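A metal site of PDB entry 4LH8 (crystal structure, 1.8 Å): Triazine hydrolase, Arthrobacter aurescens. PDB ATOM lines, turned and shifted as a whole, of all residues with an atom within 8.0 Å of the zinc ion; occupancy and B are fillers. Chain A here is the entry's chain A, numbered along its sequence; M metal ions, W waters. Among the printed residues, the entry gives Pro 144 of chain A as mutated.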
ATOM      1  N   HIS A  76      23.781 -13.660  27.058  1.00  0.00           N
ATOM      2  CA  HIS A  76      24.497 -14.818  27.597  1.00  0.00           C
ATOM      3  C   HIS A  76      25.367 -15.520  26.538  1.00  0.00           C
ATOM      4  O   HIS A  76      24.852 -16.240  25.685  1.00  0.00           O
ATOM      5  CB  HIS A  76      23.495 -15.802  28.225  1.00  0.00           C
ATOM      6  CG  HIS A  76      24.112 -16.832  29.126  1.00  0.00           C
ATOM      7  ND1 HIS A  76      24.421 -16.577  30.448  1.00  0.00           N
ATOM      8  CD2 HIS A  76      24.461 -18.115  28.896  1.00  0.00           C
ATOM      9  CE1 HIS A  76      24.936 -17.669  30.992  1.00  0.00           C
ATOM     10  NE2 HIS A  76      24.975 -18.617  30.072  1.00  0.00           N
ATOM     11  N   GLN A  77      26.677 -15.260  26.597  1.00  0.00           N
ATOM     12  CA  GLN A  77      27.663 -15.903  25.716  1.00  0.00           C
ATOM     13  C   GLN A  77      28.760 -16.605  26.531  1.00  0.00           C
ATOM     14  O   GLN A  77      28.949 -16.302  27.704  1.00  0.00           O
ATOM     15  CB  GLN A  77      28.338 -14.875  24.815  1.00  0.00           C
ATOM     16  CG  GLN A  77      27.844 -14.853  23.370  1.00  0.00           C
ATOM     17  CD  GLN A  77      28.268 -16.070  22.556  1.00  0.00           C
ATOM     18  OE1 GLN A  77      28.871 -17.023  23.076  1.00  0.00           O
ATOM     19  NE2 GLN A  77      27.945 -16.050  21.263  1.00  0.00           N
ATOM     20  N   HIS A  78      29.465 -17.546  25.893  1.00  0.00           N
ATOM     21  CA  HIS A  78      30.735 -18.063  26.403  1.00  0.00           C
ATOM     22  C   HIS A  78      31.691 -18.103  25.204  1.00  0.00           C
ATOM     23  O   HIS A  78      31.814 -19.124  24.507  1.00  0.00           O
ATOM     24  CB  HIS A  78      30.590 -19.462  27.029  1.00  0.00           C
ATOM     25  CG  HIS A  78      29.645 -19.524  28.194  1.00  0.00           C
ATOM     26  ND1 HIS A  78      29.830 -18.810  29.353  1.00  0.00           N
ATOM     27  CD2 HIS A  78      28.512 -20.238  28.377  1.00  0.00           C
ATOM     28  CE1 HIS A  78      28.851 -19.066  30.193  1.00  0.00           C
ATOM     29  NE2 HIS A  78      28.037 -19.929  29.626  1.00  0.00           N
ATOM     30  N   GLU A  81      34.211 -20.854  23.807  1.00  0.00           N
ATOM     31  CA  GLU A  81      33.648 -22.098  23.247  1.00  0.00           C
ATOM     32  C   GLU A  81      33.510 -22.078  21.730  1.00  0.00           C
ATOM     33  O   GLU A  81      33.139 -23.085  21.114  1.00  0.00           O
ATOM     34  CB  GLU A  81      32.290 -22.424  23.889  1.00  0.00           C
ATOM     35  CG  GLU A  81      32.341 -22.679  25.393  1.00  0.00           C
ATOM     36  CD  GLU A  81      30.980 -22.975  25.981  1.00  0.00           C
ATOM     37  OE1 GLU A  81      29.975 -22.910  25.239  1.00  0.00           O
ATOM     38  OE2 GLU A  81      30.905 -23.259  27.200  1.00  0.00           O
ATOM     39  N   MET A  95      23.882 -33.132  30.084  1.00  0.00           N
ATOM     40  CA  MET A  95      24.684 -32.104  30.740  1.00  0.00           C
ATOM     41  C   MET A  95      25.954 -32.647  31.368  1.00  0.00           C
ATOM     42  O   MET A  95      27.033 -32.075  31.203  1.00  0.00           O
ATOM     43  CB  MET A  95      23.865 -31.351  31.808  1.00  0.00           C
ATOM     44  CG  MET A  95      24.644 -30.269  32.571  1.00  0.00           C
ATOM     45  SD  MET A  95      25.435 -29.063  31.467  1.00  0.00           S
ATOM     46  CE  MET A  95      25.859 -27.734  32.601  1.00  0.00           C
ATOM     47  N   TRP A  98      28.466 -33.509  28.763  1.00  0.00           N
ATOM     48  CA  TRP A  98      28.830 -32.279  28.070  1.00  0.00           C
ATOM     49  C   TRP A  98      29.810 -31.455  28.893  1.00  0.00           C
ATOM     50  O   TRP A  98      30.852 -31.025  28.400  1.00  0.00           O
ATOM     51  CB  TRP A  98      27.572 -31.472  27.734  1.00  0.00           C
ATOM     52  CG  TRP A  98      27.864 -30.198  27.006  1.00  0.00           C
ATOM     53  CD1 TRP A  98      27.904 -30.022  25.646  1.00  0.00           C
ATOM     54  CD2 TRP A  98      28.152 -28.921  27.590  1.00  0.00           C
ATOM     55  NE1 TRP A  98      28.205 -28.703  25.355  1.00  0.00           N
ATOM     56  CE2 TRP A  98      28.359 -28.014  26.530  1.00  0.00           C
ATOM     57  CE3 TRP A  98      28.254 -28.457  28.899  1.00  0.00           C
ATOM     58  CZ2 TRP A  98      28.660 -26.669  26.748  1.00  0.00           C
ATOM     59  CZ3 TRP A  98      28.549 -27.124  29.116  1.00  0.00           C
ATOM     60  CH2 TRP A  98      28.753 -26.247  28.042  1.00  0.00           C
ATOM     61  N   GLN A 142      30.261 -14.456  29.563  1.00  0.00           N
ATOM     62  CA  GLN A 142      30.563 -14.980  30.892  1.00  0.00           C
ATOM     63  C   GLN A 142      31.736 -15.951  30.809  1.00  0.00           C
ATOM     64  O   GLN A 142      31.572 -17.090  30.370  1.00  0.00           O
ATOM     65  CB  GLN A 142      29.317 -15.660  31.497  1.00  0.00           C
ATOM     66  CG  GLN A 142      29.416 -15.999  32.997  1.00  0.00           C
ATOM     67  CD  GLN A 142      28.189 -16.743  33.531  1.00  0.00           C
ATOM     68  OE1 GLN A 142      27.445 -17.379  32.769  1.00  0.00           O
ATOM     69  NE2 GLN A 142      27.974 -16.669  34.846  1.00  0.00           N
ATOM     70  N   PRO A 144      34.485 -18.263  32.601  1.00  0.00           N
ATOM     71  CA  PRO A 144      34.749 -18.940  33.872  1.00  0.00           C
ATOM     72  C   PRO A 144      36.141 -19.553  33.973  1.00  0.00           C
ATOM     73  O   PRO A 144      36.488 -20.074  35.028  1.00  0.00           O
ATOM     74  CB  PRO A 144      33.731 -20.070  33.841  1.00  0.00           C
ATOM     75  CG  PRO A 144      33.706 -20.464  32.409  1.00  0.00           C
ATOM     76  CD  PRO A 144      33.864 -19.182  31.625  1.00  0.00           C
ATOM     77  N   SER A 174      33.466 -14.986  35.604  1.00  0.00           N
ATOM     78  CA  SER A 174      32.876 -16.200  36.160  1.00  0.00           C
ATOM     79  C   SER A 174      33.897 -17.056  36.886  1.00  0.00           C
ATOM     80  O   SER A 174      35.091 -16.743  36.912  1.00  0.00           O
ATOM     81  CB  SER A 174      32.174 -17.024  35.077  1.00  0.00           C
ATOM     82  OG  SER A 174      31.268 -17.946  35.666  1.00  0.00           O
ATOM     83  N   CYS A 224      29.325 -19.413  38.371  1.00  0.00           N
ATOM     84  CA  CYS A 224      28.710 -20.399  37.482  1.00  0.00           C
ATOM     85  C   CYS A 224      27.320 -20.810  37.975  1.00  0.00           C
ATOM     86  O   CYS A 224      26.380 -20.894  37.200  1.00  0.00           O
ATOM     87  CB  CYS A 224      29.599 -21.637  37.339  1.00  0.00           C
ATOM     88  SG  CYS A 224      28.980 -22.860  36.143  1.00  0.00           S
ATOM     89  N   HIS A 249      25.045 -12.003  37.860  1.00  0.00           N
ATOM     90  CA  HIS A 249      24.537 -12.970  36.886  1.00  0.00           C
ATOM     91  C   HIS A 249      24.887 -14.400  37.309  1.00  0.00           C
ATOM     92  O   HIS A 249      25.999 -14.651  37.755  1.00  0.00           O
ATOM     93  CB  HIS A 249      25.162 -12.685  35.504  1.00  0.00           C
ATOM     94  CG  HIS A 249      24.621 -13.544  34.412  1.00  0.00           C
ATOM     95  ND1 HIS A 249      23.269 -13.728  34.199  1.00  0.00           N
ATOM     96  CD2 HIS A 249      25.244 -14.259  33.439  1.00  0.00           C
ATOM     97  CE1 HIS A 249      23.091 -14.529  33.172  1.00  0.00           C
ATOM     98  NE2 HIS A 249      24.274 -14.866  32.692  1.00  0.00           N
ATOM     99  N   THR A 250      23.954 -15.325  37.154  1.00  0.00           N
ATOM    100  CA  THR A 250      24.281 -16.741  37.352  1.00  0.00           C
ATOM    101  C   THR A 250      23.320 -17.655  36.606  1.00  0.00           C
ATOM    102  O   THR A 250      22.304 -17.193  36.097  1.00  0.00           O
ATOM    103  CB  THR A 250      24.346 -17.134  38.854  1.00  0.00           C
ATOM    104  OG1 THR A 250      25.013 -18.396  38.980  1.00  0.00           O
ATOM    105  CG2 THR A 250      22.943 -17.238  39.485  1.00  0.00           C
ATOM    106  N   HIS A 251      23.665 -18.937  36.514  1.00  0.00           N
ATOM    107  CA  HIS A 251      22.778 -19.927  35.900  1.00  0.00           C
ATOM    108  C   HIS A 251      21.701 -20.286  36.913  1.00  0.00           C
ATOM    109  O   HIS A 251      21.938 -20.192  38.112  1.00  0.00           O
ATOM    110  CB  HIS A 251      23.546 -21.192  35.496  1.00  0.00           C
ATOM    111  CG  HIS A 251      24.533 -20.987  34.398  1.00  0.00           C
ATOM    112  ND1 HIS A 251      25.827 -20.567  34.632  1.00  0.00           N
ATOM    113  CD2 HIS A 251      24.423 -21.118  33.051  1.00  0.00           C
ATOM    114  CE1 HIS A 251      26.470 -20.465  33.478  1.00  0.00           C
ATOM    115  NE2 HIS A 251      25.634 -20.790  32.512  1.00  0.00           N
ATOM    116  N   GLU A 254      18.520 -25.150  36.100  1.00  0.00           N
ATOM    117  CA  GLU A 254      18.735 -26.168  35.090  1.00  0.00           C
ATOM    118  C   GLU A 254      18.267 -27.474  35.740  1.00  0.00           C
ATOM    119  O   GLU A 254      18.251 -27.573  36.969  1.00  0.00           O
ATOM    120  CB  GLU A 254      20.221 -26.237  34.732  1.00  0.00           C
ATOM    121  CG  GLU A 254      20.778 -24.868  34.319  1.00  0.00           C
ATOM    122  CD  GLU A 254      22.254 -24.892  33.963  1.00  0.00           C
ATOM    123  OE1 GLU A 254      22.954 -25.857  34.333  1.00  0.00           O
ATOM    124  OE2 GLU A 254      22.707 -23.943  33.297  1.00  0.00           O
ATOM    125  N   ALA A 286      20.204 -16.966  33.999  1.00  0.00           N
ATOM    126  CA  ALA A 286      20.269 -17.726  32.752  1.00  0.00           C
ATOM    127  C   ALA A 286      19.457 -19.033  32.762  1.00  0.00           C
ATOM    128  O   ALA A 286      19.530 -19.799  33.722  1.00  0.00           O
ATOM    129  CB  ALA A 286      21.741 -18.043  32.430  1.00  0.00           C
ATOM    130  N   HIS A 287      18.709 -19.285  31.682  1.00  0.00           N
ATOM    131  CA  HIS A 287      17.939 -20.527  31.472  1.00  0.00           C
ATOM    132  C   HIS A 287      16.605 -20.557  32.224  1.00  0.00           C
ATOM    133  O   HIS A 287      15.541 -20.444  31.617  1.00  0.00           O
ATOM    134  CB  HIS A 287      18.757 -21.793  31.810  1.00  0.00           C
ATOM    135  CG  HIS A 287      20.008 -21.956  30.992  1.00  0.00           C
ATOM    136  ND1 HIS A 287      19.999 -22.441  29.693  1.00  0.00           N
ATOM    137  CD2 HIS A 287      21.307 -21.723  31.283  1.00  0.00           C
ATOM    138  CE1 HIS A 287      21.238 -22.493  29.230  1.00  0.00           C
ATOM    139  NE2 HIS A 287      22.049 -22.056  30.183  1.00  0.00           N
ATOM    140  N   LEU A 309      17.148 -19.048  26.855  1.00  0.00           N
ATOM    141  CA  LEU A 309      18.221 -19.615  26.035  1.00  0.00           C
ATOM    142  C   LEU A 309      17.745 -20.899  25.338  1.00  0.00           C
ATOM    143  O   LEU A 309      18.132 -22.004  25.720  1.00  0.00           O
ATOM    144  CB  LEU A 309      19.463 -19.889  26.894  1.00  0.00           C
ATOM    145  CG  LEU A 309      19.917 -18.723  27.797  1.00  0.00           C
ATOM    146  CD1 LEU A 309      20.959 -19.156  28.821  1.00  0.00           C
ATOM    147  CD2 LEU A 309      20.452 -17.531  26.974  1.00  0.00           C
ATOM    148  N   PRO A 312      20.409 -24.054  23.778  1.00  0.00           N
ATOM    149  CA  PRO A 312      20.982 -25.052  24.687  1.00  0.00           C
ATOM    150  C   PRO A 312      19.926 -25.830  25.471  1.00  0.00           C
ATOM    151  O   PRO A 312      20.151 -27.007  25.765  1.00  0.00           O
ATOM    152  CB  PRO A 312      21.856 -24.209  25.629  1.00  0.00           C
ATOM    153  CG  PRO A 312      21.297 -22.841  25.559  1.00  0.00           C
ATOM    154  CD  PRO A 312      20.807 -22.684  24.128  1.00  0.00           C
ATOM    155  N   TRP A 318      16.803 -30.457  27.948  1.00  0.00           N
ATOM    156  CA  TRP A 318      16.157 -29.866  29.121  1.00  0.00           C
ATOM    157  C   TRP A 318      14.690 -29.502  28.894  1.00  0.00           C
ATOM    158  O   TRP A 318      13.874 -29.651  29.804  1.00  0.00           O
ATOM    159  CB  TRP A 318      16.906 -28.615  29.588  1.00  0.00           C
ATOM    160  CG  TRP A 318      18.266 -28.877  30.147  1.00  0.00           C
ATOM    161  CD1 TRP A 318      18.792 -30.090  30.482  1.00  0.00           C
ATOM    162  CD2 TRP A 318      19.269 -27.905  30.447  1.00  0.00           C
ATOM    163  NE1 TRP A 318      20.061 -29.929  30.983  1.00  0.00           N
ATOM    164  CE2 TRP A 318      20.371 -28.596  30.978  1.00  0.00           C
ATOM    165  CE3 TRP A 318      19.324 -26.509  30.338  1.00  0.00           C
ATOM    166  CZ2 TRP A 318      21.535 -27.945  31.390  1.00  0.00           C
ATOM    167  CZ3 TRP A 318      20.486 -25.864  30.743  1.00  0.00           C
ATOM    168  CH2 TRP A 318      21.577 -26.581  31.259  1.00  0.00           C
ATOM    169  N   THR A 337      22.268 -16.824  23.398  1.00  0.00           N
ATOM    170  CA  THR A 337      22.636 -18.022  22.649  1.00  0.00           C
ATOM    171  C   THR A 337      23.389 -19.075  23.483  1.00  0.00           C
ATOM    172  O   THR A 337      23.441 -20.260  23.115  1.00  0.00           O
ATOM    173  CB  THR A 337      23.548 -17.645  21.456  1.00  0.00           C
ATOM    174  OG1 THR A 337      24.703 -16.953  21.944  1.00  0.00           O
ATOM    175  CG2 THR A 337      22.804 -16.749  20.474  1.00  0.00           C
ATOM    176  N   THR A 338      23.937 -18.649  24.619  1.00  0.00           N
ATOM    177  CA  THR A 338      25.025 -19.338  25.329  1.00  0.00           C
ATOM    178  C   THR A 338      26.221 -19.584  24.408  1.00  0.00           C
ATOM    179  O   THR A 338      26.272 -19.041  23.304  1.00  0.00           O
ATOM    180  CB  THR A 338      24.578 -20.654  26.051  1.00  0.00           C
ATOM    181  OG1 THR A 338      24.419 -21.724  25.112  1.00  0.00           O
ATOM    182  CG2 THR A 338      23.301 -20.439  26.815  1.00  0.00           C
ATOM    183  N   GLY A 339      27.198 -20.355  24.877  1.00  0.00           N
ATOM    184  CA  GLY A 339      28.417 -20.544  24.118  1.00  0.00           C
ATOM    185  C   GLY A 339      28.250 -21.486  22.928  1.00  0.00           C
ATOM    186  O   GLY A 339      27.250 -22.190  22.837  1.00  0.00           O
ATOM    187  N   SER A 342      27.495 -25.395  23.053  1.00  0.00           N
ATOM    188  CA  SER A 342      26.131 -25.865  23.250  1.00  0.00           C
ATOM    189  C   SER A 342      25.153 -24.990  22.497  1.00  0.00           C
ATOM    190  O   SER A 342      24.229 -24.443  23.093  1.00  0.00           O
ATOM    191  CB  SER A 342      25.762 -25.928  24.740  1.00  0.00           C
ATOM    192  OG  SER A 342      25.688 -24.633  25.329  1.00  0.00           O
HETATM  193 ZN    ZN M   1      26.023 -20.501  30.377  1.00  0.00          ZN
HETATM  194  O   HOH W   1      24.611 -21.893  29.638  1.00  0.00           O
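O of Gln 142 sits at hydrogen-bond distance from ND1 of His 78 (2.7 Å). A ring nitrogen (NE2) of His 249 sits at hydrogen-bond distance from a ring nitrogen (ND1) of His 76 (2.8 Å). The backbone carbonyl oxygen of His 76 lies within hydrogen-bond range of the backbone NH of Thr 338, at 2.8 Å. O of Cys 224 sits at hydrogen-bond distance from ND1 of His 251 (2.6 Å).
The nearest printed residue that does not touch the zinc ion is Gln 142 (4.2 Å).
Water W1 binds the zinc ion. A ring nitrogen (NE2) of His 76 is bound to the zinc ion. NE2 of His 251 is bound to the zinc ion, 2.2 Å away. NE2 of His 78 is bound to the zinc ion (2.2 Å).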
